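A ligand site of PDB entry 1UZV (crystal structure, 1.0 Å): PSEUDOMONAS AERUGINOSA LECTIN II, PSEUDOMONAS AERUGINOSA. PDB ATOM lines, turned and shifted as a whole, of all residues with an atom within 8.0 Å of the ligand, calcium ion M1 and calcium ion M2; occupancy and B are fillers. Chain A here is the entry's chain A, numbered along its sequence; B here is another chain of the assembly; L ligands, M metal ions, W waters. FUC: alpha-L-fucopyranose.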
ATOM      1  N   ALA A  20      10.994   1.060  23.588  1.00  0.00           N
ATOM      2  CA  ALA A  20      10.590   0.734  22.207  1.00  0.00           C
ATOM      3  C   ALA A  20      11.802   0.600  21.289  1.00  0.00           C
ATOM      4  O   ALA A  20      12.767   1.370  21.352  1.00  0.00           O
ATOM      5  CB  ALA A  20       9.627   1.829  21.680  1.00  0.00           C
ATOM      6  N   ASN A  21      11.684  -0.375  20.385  1.00  0.00           N
ATOM      7  CA  ASN A  21      12.707  -0.649  19.376  1.00  0.00           C
ATOM      8  C   ASN A  21      12.054  -1.180  18.097  1.00  0.00           C
ATOM      9  O   ASN A  21      12.161  -2.366  17.768  1.00  0.00           O
ATOM     10  CB  ASN A  21      13.733  -1.699  19.848  1.00  0.00           C
ATOM     11  CG  ASN A  21      14.595  -1.189  20.967  1.00  0.00           C
ATOM     12  OD1 ASN A  21      15.562  -0.447  20.751  1.00  0.00           O
ATOM     13  ND2 ASN A  21      14.254  -1.605  22.179  1.00  0.00           N
ATOM     14  N   SER A  22      11.376  -0.296  17.362  1.00  0.00           N
ATOM     15  CA  SER A  22      10.586  -0.713  16.209  1.00  0.00           C
ATOM     16  C   SER A  22      10.205   0.492  15.393  1.00  0.00           C
ATOM     17  O   SER A  22      10.028   1.613  15.953  1.00  0.00           O
ATOM     18  CB  SER A  22       9.297  -1.432  16.688  1.00  0.00           C
ATOM     19  OG  SER A  22       8.476  -1.706  15.554  1.00  0.00           O
ATOM     20  N   SER A  23       9.949   0.310  14.102  1.00  0.00           N
ATOM     21  CA  SER A  23       9.332   1.359  13.287  1.00  0.00           C
ATOM     22  C   SER A  23       7.922   1.720  13.772  1.00  0.00           C
ATOM     23  O   SER A  23       7.491   2.815  13.505  1.00  0.00           O
ATOM     24  CB  SER A  23       9.278   0.855  11.819  1.00  0.00           C
ATOM     25  OG  SER A  23       8.319  -0.247  11.713  1.00  0.00           O
ATOM     26  N   GLY A  24       7.242   0.772  14.414  1.00  0.00           N
ATOM     27  CA  GLY A  24       5.817   0.964  14.732  1.00  0.00           C
ATOM     28  C   GLY A  24       5.623   1.526  16.140  1.00  0.00           C
ATOM     29  O   GLY A  24       6.393   1.274  17.063  1.00  0.00           O
ATOM     30  N   GLN A  26       4.242   1.515  19.671  1.00  0.00           N
ATOM     31  CA  GLN A  26       3.925   0.525  20.642  1.00  0.00           C
ATOM     32  C   GLN A  26       2.909   1.080  21.626  1.00  0.00           C
ATOM     33  O   GLN A  26       3.110   2.170  22.125  1.00  0.00           O
ATOM     34  CB  GLN A  26       5.169   0.071  21.431  1.00  0.00           C
ATOM     35  CG  GLN A  26       6.377  -0.263  20.558  1.00  0.00           C
ATOM     36  CD  GLN A  26       6.187  -1.523  19.764  1.00  0.00           C
ATOM     37  OE1 GLN A  26       5.907  -2.564  20.353  1.00  0.00           O
ATOM     38  NE2 GLN A  26       6.384  -1.453  18.447  1.00  0.00           N
ATOM     39  N   GLN A  43       7.034   5.585  20.002  1.00  0.00           N
ATOM     40  CA  GLN A  43       7.746   5.014  18.903  1.00  0.00           C
ATOM     41  C   GLN A  43       9.230   5.395  19.014  1.00  0.00           C
ATOM     42  O   GLN A  43       9.557   6.576  19.172  1.00  0.00           O
ATOM     43  CB  GLN A  43       7.207   5.466  17.572  1.00  0.00           C
ATOM     44  CG  GLN A  43       7.832   4.806  16.337  1.00  0.00           C
ATOM     45  CD  GLN A  43       9.134   5.382  15.865  1.00  0.00           C
ATOM     46  OE1 GLN A  43       9.296   6.613  15.810  1.00  0.00           O
ATOM     47  NE2 GLN A  43      10.076   4.539  15.520  1.00  0.00           N
ATOM     48  N   SER A  44      10.101   4.417  18.871  1.00  0.00           N
ATOM     49  CA  SER A  44      11.527   4.604  18.845  1.00  0.00           C
ATOM     50  C   SER A  44      12.198   3.420  18.215  1.00  0.00           C
ATOM     51  O   SER A  44      11.754   2.289  18.459  1.00  0.00           O
ATOM     52  CB  SER A  44      12.048   4.746  20.293  1.00  0.00           C
ATOM     53  OG  SER A  44      13.458   4.975  20.345  1.00  0.00           O
ATOM     54  N   THR A  45      13.306   3.638  17.510  1.00  0.00           N
ATOM     55  CA  THR A  45      14.249   2.583  17.149  1.00  0.00           C
ATOM     56  C   THR A  45      15.534   2.648  17.959  1.00  0.00           C
ATOM     57  O   THR A  45      16.513   2.002  17.600  1.00  0.00           O
ATOM     58  CB  THR A  45      14.524   2.546  15.659  1.00  0.00           C
ATOM     59  OG1 THR A  45      14.882   3.849  15.232  1.00  0.00           O
ATOM     60  CG2 THR A  45      13.283   2.054  14.860  1.00  0.00           C
ATOM     61  N   VAL A  69       0.505  -3.260  18.482  1.00  0.00           N
ATOM     62  CA  VAL A  69       1.166  -2.447  17.444  1.00  0.00           C
ATOM     63  C   VAL A  69       0.343  -2.559  16.192  1.00  0.00           C
ATOM     64  O   VAL A  69       0.000  -3.675  15.779  1.00  0.00           O
ATOM     65  CB  VAL A  69       2.605  -2.913  17.187  1.00  0.00           C
ATOM     66  CG1 VAL A  69       3.287  -2.003  16.152  1.00  0.00           C
ATOM     67  CG2 VAL A  69       3.432  -3.034  18.445  1.00  0.00           C
ATOM     68  N   SER A  94       8.580  -8.482  23.209  1.00  0.00           N
ATOM     69  CA  SER A  94       7.448  -8.613  22.308  1.00  0.00           C
ATOM     70  C   SER A  94       7.909  -8.429  20.875  1.00  0.00           C
ATOM     71  O   SER A  94       8.854  -7.684  20.590  1.00  0.00           O
ATOM     72  CB  SER A  94       6.359  -7.593  22.691  1.00  0.00           C
ATOM     73  OG  SER A  94       6.793  -6.270  22.482  1.00  0.00           O
ATOM     74  N   GLU A  95       7.198  -9.099  19.977  1.00  0.00           N
ATOM     75  CA  GLU A  95       7.494  -9.078  18.543  1.00  0.00           C
ATOM     76  C   GLU A  95       6.244  -8.634  17.774  1.00  0.00           C
ATOM     77  O   GLU A  95       5.196  -9.276  17.872  1.00  0.00           O
ATOM     78  CB  GLU A  95       7.937 -10.481  18.083  1.00  0.00           C
ATOM     79  CG  GLU A  95       8.232 -10.530  16.588  1.00  0.00           C
ATOM     80  CD  GLU A  95       9.266  -9.522  16.126  1.00  0.00           C
ATOM     81  OE1 GLU A  95      10.330  -9.371  16.790  1.00  0.00           O
ATOM     82  OE2 GLU A  95       8.996  -8.780  15.143  1.00  0.00           O
ATOM     83  N   ASP A  96       6.425  -7.581  16.981  1.00  0.00           N
ATOM     84  CA  ASP A  96       5.323  -6.982  16.229  1.00  0.00           C
ATOM     85  C   ASP A  96       5.395  -7.269  14.729  1.00  0.00           C
ATOM     86  O   ASP A  96       4.525  -6.826  13.982  1.00  0.00           O
ATOM     87  CB  ASP A  96       5.314  -5.454  16.422  1.00  0.00           C
ATOM     88  CG  ASP A  96       6.481  -4.680  15.835  1.00  0.00           C
ATOM     89  OD1 ASP A  96       7.130  -5.145  14.893  1.00  0.00           O
ATOM     90  OD2 ASP A  96       6.755  -3.547  16.353  1.00  0.00           O
ATOM     91  N   GLY A  97       6.433  -8.011  14.305  1.00  0.00           N
ATOM     92  CA  GLY A  97       6.729  -8.213  12.939  1.00  0.00           C
ATOM     93  C   GLY A  97       7.256  -9.605  12.626  1.00  0.00           C
ATOM     94  O   GLY A  97       6.741 -10.580  13.190  1.00  0.00           O
ATOM     95  N   THR A  98       8.263  -9.657  11.764  1.00  0.00           N
ATOM     96  CA  THR A  98       8.723 -10.899  11.191  1.00  0.00           C
ATOM     97  C   THR A  98      10.187 -11.252  11.530  1.00  0.00           C
ATOM     98  O   THR A  98      10.598 -12.370  11.221  1.00  0.00           O
ATOM     99  CB  THR A  98       8.559 -10.898   9.641  1.00  0.00           C
ATOM    100  OG1 THR A  98       9.323  -9.819   9.092  1.00  0.00           O
ATOM    101  CG2 THR A  98       7.080 -10.714   9.291  1.00  0.00           C
ATOM    102  N   ASP A  99      10.955 -10.344  12.096  1.00  0.00           N
ATOM    103  CA  ASP A  99      12.362 -10.529  12.291  1.00  0.00           C
ATOM    104  C   ASP A  99      12.699 -11.311  13.584  1.00  0.00           C
ATOM    105  O   ASP A  99      13.808 -11.745  13.775  1.00  0.00           O
ATOM    106  CB  ASP A  99      13.168  -9.258  12.227  1.00  0.00           C
ATOM    107  CG  ASP A  99      12.898  -8.252  13.335  1.00  0.00           C
ATOM    108  OD1 ASP A  99      11.945  -8.437  14.061  1.00  0.00           O
ATOM    109  OD2 ASP A  99      13.737  -7.268  13.452  1.00  0.00           O
ATOM    110  N   ASN A 100      11.744 -11.466  14.475  1.00  0.00           N
ATOM    111  CA  ASN A 100      11.924 -12.221  15.703  1.00  0.00           C
ATOM    112  C   ASN A 100      13.037 -11.725  16.591  1.00  0.00           C
ATOM    113  O   ASN A 100      13.717 -12.499  17.252  1.00  0.00           O
ATOM    114  CB  ASN A 100      12.017 -13.707  15.377  1.00  0.00           C
ATOM    115  CG  ASN A 100      10.668 -14.149  14.796  1.00  0.00           C
ATOM    116  OD1 ASN A 100       9.617 -13.615  15.148  1.00  0.00           O
ATOM    117  ND2 ASN A 100      10.755 -15.146  13.938  1.00  0.00           N
ATOM    118  N   ASP A 101      13.220 -10.388  16.654  1.00  0.00           N
ATOM    119  CA  ASP A 101      14.134  -9.791  17.620  1.00  0.00           C
ATOM    120  C   ASP A 101      13.488  -9.663  19.017  1.00  0.00           C
ATOM    121  O   ASP A 101      14.218  -9.590  20.026  1.00  0.00           O
ATOM    122  CB  ASP A 101      14.824  -8.514  17.151  1.00  0.00           C
ATOM    123  CG  ASP A 101      13.944  -7.310  16.892  1.00  0.00           C
ATOM    124  OD1 ASP A 101      12.692  -7.416  16.995  1.00  0.00           O
ATOM    125  OD2 ASP A 101      14.504  -6.221  16.588  1.00  0.00           O
ATOM    126  N   TYR A 102      12.166  -9.661  19.118  1.00  0.00           N
ATOM    127  CA  TYR A 102      11.455  -9.635  20.406  1.00  0.00           C
ATOM    128  C   TYR A 102      11.801  -8.453  21.285  1.00  0.00           C
ATOM    129  O   TYR A 102      11.557  -8.487  22.484  1.00  0.00           O
ATOM    130  CB  TYR A 102      11.573 -11.002  21.163  1.00  0.00           C
ATOM    131  CG  TYR A 102      10.589 -11.977  20.559  1.00  0.00           C
ATOM    132  CD1 TYR A 102       9.299 -12.102  21.056  1.00  0.00           C
ATOM    133  CD2 TYR A 102      10.869 -12.742  19.438  1.00  0.00           C
ATOM    134  CE1 TYR A 102       8.369 -12.963  20.528  1.00  0.00           C
ATOM    135  CE2 TYR A 102       9.942 -13.582  18.869  1.00  0.00           C
ATOM    136  CZ  TYR A 102       8.690 -13.682  19.428  1.00  0.00           C
ATOM    137  OH  TYR A 102       7.762 -14.501  18.795  1.00  0.00           O
ATOM    138  N   ASN A 103      12.252  -7.340  20.670  1.00  0.00           N
ATOM    139  CA  ASN A 103      12.588  -6.166  21.433  1.00  0.00           C
ATOM    140  C   ASN A 103      11.670  -4.987  21.113  1.00  0.00           C
ATOM    141  O   ASN A 103      11.970  -3.846  21.503  1.00  0.00           O
ATOM    142  CB  ASN A 103      14.065  -5.751  21.240  1.00  0.00           C
ATOM    143  CG  ASN A 103      14.290  -5.180  19.837  1.00  0.00           C
ATOM    144  OD1 ASN A 103      13.371  -5.103  19.042  1.00  0.00           O
ATOM    145  ND2 ASN A 103      15.503  -4.746  19.551  1.00  0.00           N
ATOM    146  N   ASP A 104      10.599  -5.237  20.397  1.00  0.00           N
ATOM    147  CA  ASP A 104       9.887  -4.118  19.762  1.00  0.00           C
ATOM    148  C   ASP A 104       9.251  -3.243  20.823  1.00  0.00           C
ATOM    149  O   ASP A 104       9.280  -2.008  20.722  1.00  0.00           O
ATOM    150  CB  ASP A 104       8.903  -4.697  18.755  1.00  0.00           C
ATOM    151  CG  ASP A 104       9.572  -5.423  17.638  1.00  0.00           C
ATOM    152  OD1 ASP A 104      10.695  -5.069  17.193  1.00  0.00           O
ATOM    153  OD2 ASP A 104       8.987  -6.442  17.156  1.00  0.00           O
ATOM    154  N   ALA A 105       8.696  -3.886  21.846  1.00  0.00           N
ATOM    155  CA  ALA A 105       8.474  -3.269  23.151  1.00  0.00           C
ATOM    156  C   ALA A 105       9.143  -4.206  24.165  1.00  0.00           C
ATOM    157  O   ALA A 105       8.902  -5.426  24.093  1.00  0.00           O
ATOM    158  CB  ALA A 105       7.033  -3.056  23.538  1.00  0.00           C
ATOM    159  N   GLU B  86      17.348 -15.097  22.076  1.00  0.00           N
ATOM    160  CA  GLU B  86      17.600 -13.871  21.320  1.00  0.00           C
ATOM    161  C   GLU B  86      17.629 -12.583  22.141  1.00  0.00           C
ATOM    162  O   GLU B  86      18.395 -11.678  21.814  1.00  0.00           O
ATOM    163  CB  GLU B  86      16.509 -13.693  20.248  1.00  0.00           C
ATOM    164  CG  GLU B  86      16.322 -12.289  19.678  1.00  0.00           C
ATOM    165  CD  GLU B  86      17.460 -11.912  18.739  1.00  0.00           C
ATOM    166  OE1 GLU B  86      18.304 -12.816  18.462  1.00  0.00           O
ATOM    167  OE2 GLU B  86      17.440 -10.730  18.345  1.00  0.00           O
ATOM    168  N   PRO B 112      19.453  -7.116  21.895  1.00  0.00           N
ATOM    169  CA  PRO B 112      19.782  -6.057  20.946  1.00  0.00           C
ATOM    170  C   PRO B 112      18.748  -4.929  20.948  1.00  0.00           C
ATOM    171  O   PRO B 112      17.615  -5.082  21.469  1.00  0.00           O
ATOM    172  CB  PRO B 112      19.747  -6.756  19.592  1.00  0.00           C
ATOM    173  CG  PRO B 112      18.704  -7.801  19.773  1.00  0.00           C
ATOM    174  CD  PRO B 112      18.882  -8.285  21.192  1.00  0.00           C
ATOM    175  N   LEU B 113      19.120  -3.817  20.353  1.00  0.00           N
ATOM    176  CA  LEU B 113      18.273  -2.637  20.114  1.00  0.00           C
ATOM    177  C   LEU B 113      17.840  -2.587  18.655  1.00  0.00           C
ATOM    178  O   LEU B 113      18.283  -3.363  17.840  1.00  0.00           O
ATOM    179  CB  LEU B 113      18.985  -1.370  20.502  1.00  0.00           C
ATOM    180  CG  LEU B 113      19.544  -1.332  21.921  1.00  0.00           C
ATOM    181  CD1 LEU B 113      20.059   0.068  22.241  1.00  0.00           C
ATOM    182  CD2 LEU B 113      18.512  -1.782  22.974  1.00  0.00           C
ATOM    183  N   GLY B 114      16.982  -1.627  18.367  1.00  0.00           N
ATOM    184  CA  GLY B 114      16.603  -1.302  17.010  1.00  0.00           C
ATOM    185  C   GLY B 114      15.406  -2.093  16.458  1.00  0.00           C
ATOM    186  O   GLY B 114      14.996  -3.160  16.980  1.00  0.00           O
ATOM    187  OXT GLY B 114      14.904  -1.617  15.375  1.00  0.00           O
HETATM  188  C1  FUC L   1       9.889  -3.406  12.951  1.00  0.00           C
HETATM  189  C2  FUC L   1      10.400  -4.365  13.994  1.00  0.00           C
HETATM  190  C3  FUC L   1      11.826  -4.699  13.689  1.00  0.00           C
HETATM  191  C4  FUC L   1      12.701  -3.485  13.542  1.00  0.00           C
HETATM  192  C5  FUC L   1      12.094  -2.525  12.544  1.00  0.00           C
HETATM  193  C6  FUC L   1      12.827  -1.186  12.469  1.00  0.00           C
HETATM  194  O1  FUC L   1       9.802  -4.090  11.717  1.00  0.00           O
HETATM  195  O2  FUC L   1       9.649  -5.572  14.113  1.00  0.00           O
HETATM  196  O3  FUC L   1      12.316  -5.565  14.735  1.00  0.00           O
HETATM  197  O4  FUC L   1      12.788  -2.922  14.882  1.00  0.00           O
HETATM  198  O5  FUC L   1      10.681  -2.244  12.895  1.00  0.00           O
HETATM  199 CA    CA M   1      10.744  -7.214  15.675  1.00  0.00          CA
HETATM  200 CA    CA M   2      12.929  -4.423  16.851  1.00  0.00          CA
HETATM  201  O   HOH W   1       9.851  -7.243  11.632  1.00  0.00           O
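The backbone NH of Ser 23 lies within hydrogen-bond range of an oxygen (O5) of the ligand (2.9 Å).
The side-chain carboxylate (OD1) of Asp 96 lies close to an oxygen (O2) of the ligand.
The side-chain hydroxyl (OG) of Ser 22 sits close to an oxygen (O5) of the ligand (3.5 Å).
O5 of the ligand lies within hydrogen-bond range of OG of Ser 23, at 3.3 Å.
The side-chain carboxylate (OD2) of Asp 104 sits close to the backbone NH (N) of Asp 96 (2.8 Å).
N of Tyr 102 sits close to OE1 of Glu 95, 3.0 Å away.
The backbone NH (N) of Gly 24 sits at hydrogen-bond distance from the side-chain hydroxyl (OG) of Ser 22 (3.0 Å).
The backbone NH (N) of Asn 103 is in hydrogen-bond range of the backbone carbonyl oxygen (O) of Ser 94, at 3.4 Å.
OD2 of Asp 96 lies within hydrogen-bond range of OG of Ser 22 (2.6 Å).
The side-chain carboxylate (OE2) of Glu 95 lies close to the backbone NH (N) of Gly 97.
OE1 of Glu 95 sits close to N of Asn 100 (3.4 Å).
The side-chain carboxylate (OD2) of Asp 96 lies within hydrogen-bond range of the side-chain amide nitrogen (NE2) of Gln 26.
Of the 26 residues printed, 9 come within 4 Å of the ligand.
Of the 26 residues printed, 4 come within 4 Å of calcium ion M1.
Of the 26 residues printed, 5 come within 4 Å of calcium ion M2.
Calcium ion M1 is bound by the side-chain carboxylate (OD1) of Asp 99 (2.4 Å), the side-chain carboxylate (OD1) of Asp 101 (2.4 Å), the side-chain carboxylate (OE2) of Glu 95 (2.4 Å), the side-chain carboxylate (OD2) of Asp 104 (2.4 Å), the side-chain carboxylate (OE1) of Glu 95 (2.5 Å), an oxygen (O3) of the ligand (2.5 Å), an oxygen (O2) of the ligand (2.5 Å) and the side-chain carboxylate (OD1) of Asp 104 (2.6 Å).
Calcium ion M2 is bound by the side-chain amide oxygen (OD1) of Asn 103 (2.3 Å), the side-chain carboxylate (OD1) of Asp 104 (2.4 Å), the backbone carbonyl oxygen (O) of Asn 21 (2.4 Å), the side-chain carboxylate (OD2) of Asp 101 (2.4 Å), the chain-end carboxylate (O) of Gly 114 of chain B (2.4 Å), an oxygen (O4) of the ligand (2.5 Å) and an oxygen (O3) of the ligand (2.5 Å).
Calcium ion M2 has seven donor atoms within binding distance.
Slightly farther from calcium ion M2 lies the side-chain carboxylate (OD1) of Asp 101 (3.0 Å).
Water W1 lies within hydrogen-bond range of the backbone NH of Thr 98 (2.9 Å), an oxygen (O1) of the ligand (3.2 Å) and the backbone NH of Asp 99 (3.3 Å).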
